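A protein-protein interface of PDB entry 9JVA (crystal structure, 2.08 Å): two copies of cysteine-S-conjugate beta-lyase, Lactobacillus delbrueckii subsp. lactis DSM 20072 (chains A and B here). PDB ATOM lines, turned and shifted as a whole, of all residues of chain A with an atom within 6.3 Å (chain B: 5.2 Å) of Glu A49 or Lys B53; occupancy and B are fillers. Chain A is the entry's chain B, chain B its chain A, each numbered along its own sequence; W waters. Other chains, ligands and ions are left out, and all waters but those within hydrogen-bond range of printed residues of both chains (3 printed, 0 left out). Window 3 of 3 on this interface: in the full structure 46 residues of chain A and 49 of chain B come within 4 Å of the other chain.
Glu A49 touches Leu B52, and with the chains exchanged Leu A52 touches Glu B49.
Glu A49 touches Lys B53, but with the chains exchanged Lys A53 does not touch Glu B49 (5.0 Å).
Leu B52 touches its own counterpart, Leu A52.
The side-chain sulfur of Met A45 lies close to the backbone carbonyl oxygen of Leu B52 (3.6 Å).
The side-chain amino group of Lys B53 lies within salt-bridge range of the side-chain carboxylate of Glu A49 (2.8 Å).
Lys A13 touches Val B54 (O to CG1, 3.4 Å).
Arg A39 touches Ala B55 (CA to O, 3.2 Å).
Met A45 touches Ala B55.
CD1 of Leu B52 touches CB of Met A48, at 3.6 Å.
CG of Glu A49 touches CD1 of Leu B52, 3.9 Å away.
OE1 of Glu B49 touches CB of Leu A52, at 3.6 Å.
Leu A52 touches Leu B52.
Leu A271 touches Leu B52.
Water W2 lies within hydrogen-bond range of the side-chain carboxylate of Glu B49 (2.4 Å), the side-chain carboxylate of Glu A49 (3.0 Å) and the side-chain amino group of Lys B53 (3.5 Å).
Water W3 bridges the backbone carbonyl oxygen of Lys B53 (2.8 Å) and the guanidinium group of Arg A39 (3.4 Å).
Water W1 bridges O of Val B54 (2.8 Å) and N of Lys A13 (3.2 Å).
Hydrophobic or aromatic side chains of chain B that line the printed part of chain A: Leu B52, Val B54 and Ala B55.
Of the 14 printed residues of chain A, 7 touch a printed residue of chain B.
Among the printed residues, 10 pairs touch across the chains.
Among the printed residues, Asp or Glu carboxylates within 4 Å of a Lys or Arg side-chain nitrogen of the other chain: Glu A49 with Lys B53.
Glu A49 touches two residues of chain B.
Lys B53 touches just one residue of chain A: Glu A49 (2.8 Å).
Of the printed residues of chain A, Glu B49 touches Leu A52 (3.6 Å).
Of the printed residues of chain B, Lys A13 touches Val B54 (3.4 Å).
The nearest residue of chain B that does not touch Glu A49 is Glu B49 (4.4 Å).
The nearest residue of chain A that does not touch Lys B53 is Arg A39 (4.9 Å).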
ATOM      1  N   LYS A  13      11.331 -18.212  21.357  1.00  0.00           N
ATOM      2  CA  LYS A  13      11.767 -18.328  19.971  1.00  0.00           C
ATOM      3  C   LYS A  13      12.323 -16.983  19.519  1.00  0.00           C
ATOM      4  O   LYS A  13      11.601 -15.977  19.505  1.00  0.00           O
ATOM      5  CB  LYS A  13      10.615 -18.778  19.069  1.00  0.00           C
ATOM      6  CG  LYS A  13      10.458 -20.294  19.009  1.00  0.00           C
ATOM      7  CD  LYS A  13       8.997 -20.756  18.957  1.00  0.00           C
ATOM      8  CE  LYS A  13       8.778 -21.999  19.834  1.00  0.00           C
ATOM      9  NZ  LYS A  13       9.708 -23.123  19.475  1.00  0.00           N
ATOM     10  N   ARG A  39      11.339 -16.817  29.211  1.00  0.00           N
ATOM     11  CA  ARG A  39      10.648 -15.557  28.963  1.00  0.00           C
ATOM     12  C   ARG A  39      10.890 -14.598  30.125  1.00  0.00           C
ATOM     13  O   ARG A  39      11.032 -15.013  31.275  1.00  0.00           O
ATOM     14  CB  ARG A  39       9.141 -15.791  28.822  1.00  0.00           C
ATOM     15  CG  ARG A  39       8.735 -16.842  27.805  1.00  0.00           C
ATOM     16  CD  ARG A  39       7.262 -17.192  27.995  1.00  0.00           C
ATOM     17  NE  ARG A  39       6.497 -16.046  28.501  1.00  0.00           N
ATOM     18  CZ  ARG A  39       6.042 -15.049  27.737  1.00  0.00           C
ATOM     19  NH1 ARG A  39       6.282 -15.053  26.429  1.00  0.00           N
ATOM     20  NH2 ARG A  39       5.348 -14.044  28.275  1.00  0.00           N
ATOM     21  N   ILE A  44       7.618  -6.801  33.381  1.00  0.00           N
ATOM     22  CA  ILE A  44       8.530  -6.023  32.543  1.00  0.00           C
ATOM     23  C   ILE A  44       7.968  -5.895  31.136  1.00  0.00           C
ATOM     24  O   ILE A  44       7.993  -4.810  30.538  1.00  0.00           O
ATOM     25  CB  ILE A  44       9.938  -6.653  32.533  1.00  0.00           C
ATOM     26  CG1 ILE A  44      10.417  -6.886  33.965  1.00  0.00           C
ATOM     27  CG2 ILE A  44      10.932  -5.775  31.749  1.00  0.00           C
ATOM     28  CD1 ILE A  44      11.716  -7.683  34.072  1.00  0.00           C
ATOM     29  N   MET A  45       7.445  -6.999  30.587  1.00  0.00           N
ATOM     30  CA  MET A  45       6.828  -6.959  29.263  1.00  0.00           C
ATOM     31  C   MET A  45       5.709  -5.938  29.204  1.00  0.00           C
ATOM     32  O   MET A  45       5.576  -5.216  28.210  1.00  0.00           O
ATOM     33  CB  MET A  45       6.271  -8.332  28.888  1.00  0.00           C
ATOM     34  CG  MET A  45       7.295  -9.317  28.364  1.00  0.00           C
ATOM     35  SD  MET A  45       7.920  -8.877  26.723  1.00  0.00           S
ATOM     36  CE  MET A  45       6.477  -8.074  26.033  1.00  0.00           C
ATOM     37  N   THR A  46       4.883  -5.876  30.251  1.00  0.00           N
ATOM     38  CA  THR A  46       3.797  -4.899  30.282  1.00  0.00           C
ATOM     39  C   THR A  46       4.332  -3.477  30.165  1.00  0.00           C
ATOM     40  O   THR A  46       3.744  -2.640  29.464  1.00  0.00           O
ATOM     41  CB  THR A  46       2.983  -5.041  31.565  1.00  0.00           C
ATOM     42  OG1 THR A  46       2.397  -6.343  31.616  1.00  0.00           O
ATOM     43  CG2 THR A  46       1.871  -3.993  31.614  1.00  0.00           C
ATOM     44  N   SER A  47       5.454  -3.187  30.836  1.00  0.00           N
ATOM     45  CA  SER A  47       6.008  -1.833  30.800  1.00  0.00           C
ATOM     46  C   SER A  47       6.522  -1.484  29.408  1.00  0.00           C
ATOM     47  O   SER A  47       6.322  -0.363  28.925  1.00  0.00           O
ATOM     48  CB  SER A  47       7.130  -1.693  31.829  1.00  0.00           C
ATOM     49  OG  SER A  47       8.316  -2.360  31.392  1.00  0.00           O
ATOM     50  N   MET A  48       7.177  -2.439  28.748  1.00  0.00           N
ATOM     51  CA  MET A  48       7.671  -2.203  27.399  1.00  0.00           C
ATOM     52  C   MET A  48       6.528  -1.950  26.421  1.00  0.00           C
ATOM     53  O   MET A  48       6.588  -1.011  25.618  1.00  0.00           O
ATOM     54  CB  MET A  48       8.522  -3.386  26.952  1.00  0.00           C
ATOM     55  CG  MET A  48       9.767  -3.578  27.809  1.00  0.00           C
ATOM     56  SD  MET A  48      10.635  -4.987  27.134  1.00  0.00           S
ATOM     57  CE  MET A  48      12.091  -5.084  28.161  1.00  0.00           C
ATOM     58  N   GLU A  49       5.486  -2.752  26.477  1.00  0.00           N
ATOM     59  CA  GLU A  49       4.337  -2.599  25.556  1.00  0.00           C
ATOM     60  C   GLU A  49       3.632  -1.258  25.802  1.00  0.00           C
ATOM     61  O   GLU A  49       3.195  -0.654  24.831  1.00  0.00           O
ATOM     62  CB  GLU A  49       3.464  -3.851  25.643  1.00  0.00           C
ATOM     63  CG  GLU A  49       4.135  -5.034  24.980  1.00  0.00           C
ATOM     64  CD  GLU A  49       3.470  -6.392  25.082  1.00  0.00           C
ATOM     65  OE1 GLU A  49       2.838  -6.674  26.112  1.00  0.00           O
ATOM     66  OE2 GLU A  49       3.624  -7.178  24.135  1.00  0.00           O
ATOM     67  N   GLU A  50       3.551  -0.807  27.042  1.00  0.00           N
ATOM     68  CA  GLU A  50       2.941   0.507  27.370  1.00  0.00           C
ATOM     69  C   GLU A  50       3.789   1.638  26.768  1.00  0.00           C
ATOM     70  O   GLU A  50       3.246   2.581  26.240  1.00  0.00           O
ATOM     71  CB  GLU A  50       2.815   0.646  28.882  1.00  0.00           C
ATOM     72  CG  GLU A  50       2.394   2.013  29.364  1.00  0.00           C
ATOM     73  CD  GLU A  50       0.978   2.344  28.950  1.00  0.00           C
ATOM     74  OE1 GLU A  50       0.710   3.522  28.680  1.00  0.00           O
ATOM     75  OE2 GLU A  50       0.161   1.413  28.888  1.00  0.00           O
ATOM     76  N   LYS A  51       5.095   1.506  26.879  1.00  0.00           N
ATOM     77  CA  LYS A  51       5.950   2.557  26.340  1.00  0.00           C
ATOM     78  C   LYS A  51       5.792   2.676  24.831  1.00  0.00           C
ATOM     79  O   LYS A  51       5.818   3.784  24.282  1.00  0.00           O
ATOM     80  CB  LYS A  51       7.410   2.280  26.704  1.00  0.00           C
ATOM     81  CG  LYS A  51       8.428   3.287  26.132  1.00  0.00           C
ATOM     82  CD  LYS A  51       8.110   4.737  26.540  1.00  0.00           C
ATOM     83  CE  LYS A  51       9.121   5.710  25.951  1.00  0.00           C
ATOM     84  NZ  LYS A  51      10.428   5.589  26.662  1.00  0.00           N
ATOM     85  N   LEU A  52       5.633   1.547  24.136  1.00  0.00           N
ATOM     86  CA  LEU A  52       5.498   1.605  22.684  1.00  0.00           C
ATOM     87  C   LEU A  52       4.234   2.331  22.255  1.00  0.00           C
ATOM     88  O   LEU A  52       4.166   2.802  21.117  1.00  0.00           O
ATOM     89  CB  LEU A  52       5.503   0.198  22.076  1.00  0.00           C
ATOM     90  CG  LEU A  52       6.801  -0.606  22.090  1.00  0.00           C
ATOM     91  CD1 LEU A  52       6.707  -1.728  21.084  1.00  0.00           C
ATOM     92  CD2 LEU A  52       8.012   0.260  21.805  1.00  0.00           C
ATOM     93  N   LYS A  53       3.256   2.445  23.140  1.00  0.00           N
ATOM     94  CA  LYS A  53       2.012   3.194  22.823  1.00  0.00           C
ATOM     95  C   LYS A  53       2.313   4.678  22.558  1.00  0.00           C
ATOM     96  O   LYS A  53       1.477   5.322  21.959  1.00  0.00           O
ATOM     97  CB  LYS A  53       1.011   3.087  23.971  1.00  0.00           C
ATOM     98  CG  LYS A  53       0.326   1.737  24.093  1.00  0.00           C
ATOM     99  CD  LYS A  53      -0.081   1.419  25.507  1.00  0.00           C
ATOM    100  CE  LYS A  53      -1.485   1.858  25.848  1.00  0.00           C
ATOM    101  NZ  LYS A  53      -2.002   1.140  27.035  1.00  0.00           N
ATOM    102  N   VAL A  54       3.465   5.175  23.006  1.00  0.00           N
ATOM    103  CA  VAL A  54       3.786   6.569  22.712  1.00  0.00           C
ATOM    104  C   VAL A  54       3.846   6.778  21.203  1.00  0.00           C
ATOM    105  O   VAL A  54       3.382   7.801  20.685  1.00  0.00           O
ATOM    106  CB  VAL A  54       5.097   6.992  23.408  1.00  0.00           C
ATOM    107  CG1 VAL A  54       5.410   8.455  23.085  1.00  0.00           C
ATOM    108  CG2 VAL A  54       4.990   6.805  24.921  1.00  0.00           C
ATOM    109  N   LEU A 271      13.401   2.087  25.582  1.00  0.00           N
ATOM    110  CA  LEU A 271      12.806   1.141  26.518  1.00  0.00           C
ATOM    111  C   LEU A 271      13.522   1.059  27.858  1.00  0.00           C
ATOM    112  O   LEU A 271      12.930   0.572  28.827  1.00  0.00           O
ATOM    113  CB  LEU A 271      12.756  -0.265  25.893  1.00  0.00           C
ATOM    114  CG  LEU A 271      11.686  -0.466  24.810  1.00  0.00           C
ATOM    115  CD1 LEU A 271      11.618  -1.944  24.426  1.00  0.00           C
ATOM    116  CD2 LEU A 271      10.311   0.043  25.268  1.00  0.00           C
ATOM    117  N   GLU B  49       6.680  -3.800  17.846  1.00  0.00           N
ATOM    118  CA  GLU B  49       5.685  -4.593  18.555  1.00  0.00           C
ATOM    119  C   GLU B  49       5.906  -6.077  18.348  1.00  0.00           C
ATOM    120  O   GLU B  49       5.798  -6.866  19.294  1.00  0.00           O
ATOM    121  CB  GLU B  49       4.276  -4.197  18.117  1.00  0.00           C
ATOM    122  CG  GLU B  49       3.937  -2.863  18.695  1.00  0.00           C
ATOM    123  CD  GLU B  49       3.287  -2.991  20.057  1.00  0.00           C
ATOM    124  OE1 GLU B  49       2.990  -1.876  20.628  1.00  0.00           O
ATOM    125  OE2 GLU B  49       3.083  -4.093  20.592  1.00  0.00           O
ATOM    126  N   GLU B  50       6.245  -6.474  17.127  1.00  0.00           N
ATOM    127  CA  GLU B  50       6.488  -7.882  16.863  1.00  0.00           C
ATOM    128  C   GLU B  50       7.773  -8.366  17.522  1.00  0.00           C
ATOM    129  O   GLU B  50       7.838  -9.517  17.977  1.00  0.00           O
ATOM    130  CB  GLU B  50       6.525  -8.122  15.360  1.00  0.00           C
ATOM    131  CG  GLU B  50       5.151  -7.926  14.704  1.00  0.00           C
ATOM    132  CD  GLU B  50       5.236  -7.740  13.202  1.00  0.00           C
ATOM    133  OE1 GLU B  50       6.367  -7.645  12.670  1.00  0.00           O
ATOM    134  OE2 GLU B  50       4.164  -7.665  12.552  1.00  0.00           O
ATOM    135  N   LYS B  51       8.800  -7.515  17.587  1.00  0.00           N
ATOM    136  CA  LYS B  51      10.048  -7.933  18.230  1.00  0.00           C
ATOM    137  C   LYS B  51       9.859  -8.128  19.731  1.00  0.00           C
ATOM    138  O   LYS B  51      10.469  -9.023  20.325  1.00  0.00           O
ATOM    139  CB  LYS B  51      11.152  -6.911  17.949  1.00  0.00           C
ATOM    140  CG  LYS B  51      12.461  -7.139  18.730  1.00  0.00           C
ATOM    141  CD  LYS B  51      13.131  -8.464  18.369  1.00  0.00           C
ATOM    142  CE  LYS B  51      14.473  -8.665  19.088  1.00  0.00           C
ATOM    143  NZ  LYS B  51      15.556  -7.773  18.554  1.00  0.00           N
ATOM    144  N   LEU B  52       9.006  -7.313  20.367  1.00  0.00           N
ATOM    145  CA  LEU B  52       8.760  -7.490  21.795  1.00  0.00           C
ATOM    146  C   LEU B  52       8.131  -8.844  22.100  1.00  0.00           C
ATOM    147  O   LEU B  52       8.282  -9.368  23.211  1.00  0.00           O
ATOM    148  CB  LEU B  52       7.866  -6.371  22.322  1.00  0.00           C
ATOM    149  CG  LEU B  52       8.525  -5.003  22.531  1.00  0.00           C
ATOM    150  CD1 LEU B  52       7.680  -4.179  23.505  1.00  0.00           C
ATOM    151  CD2 LEU B  52       9.970  -5.129  23.029  1.00  0.00           C
ATOM    152  N   LYS B  53       7.466  -9.431  21.128  1.00  0.00           N
ATOM    153  CA  LYS B  53       6.799 -10.739  21.343  1.00  0.00           C
ATOM    154  C   LYS B  53       7.813 -11.857  21.606  1.00  0.00           C
ATOM    155  O   LYS B  53       7.408 -12.879  22.128  1.00  0.00           O
ATOM    156  CB  LYS B  53       5.911 -11.037  20.134  1.00  0.00           C
ATOM    157  CG  LYS B  53       4.715 -10.115  19.965  1.00  0.00           C
ATOM    158  CD  LYS B  53       3.894  -9.955  21.220  1.00  0.00           C
ATOM    159  CE  LYS B  53       2.675  -9.087  20.997  1.00  0.00           C
ATOM    160  NZ  LYS B  53       2.109  -8.591  22.270  1.00  0.00           N
ATOM    161  N   VAL B  54       9.075 -11.674  21.236  1.00  0.00           N
ATOM    162  CA  VAL B  54      10.078 -12.686  21.576  1.00  0.00           C
ATOM    163  C   VAL B  54      10.130 -12.900  23.087  1.00  0.00           C
ATOM    164  O   VAL B  54      10.383 -14.017  23.556  1.00  0.00           O
ATOM    165  CB  VAL B  54      11.467 -12.295  21.019  1.00  0.00           C
ATOM    166  CG1 VAL B  54      12.512 -13.344  21.410  1.00  0.00           C
ATOM    167  CG2 VAL B  54      11.437 -12.129  19.504  1.00  0.00           C
ATOM    168  N   ALA B  55       9.881 -11.845  23.865  1.00  0.00           N
ATOM    169  CA  ALA B  55       9.793 -11.905  25.327  1.00  0.00           C
ATOM    170  C   ALA B  55      11.077 -12.430  25.963  1.00  0.00           C
ATOM    171  O   ALA B  55      11.050 -12.980  27.065  1.00  0.00           O
ATOM    172  CB  ALA B  55       8.598 -12.737  25.798  1.00  0.00           C
HETATM  173  O   HOH W   1       9.025 -16.053  22.116  1.00  0.00           O
HETATM  174  O   HOH W   2       4.269  -6.022  21.468  1.00  0.00           O
HETATM  175  O   HOH W   3       5.167 -13.152  23.795  1.00  0.00           O
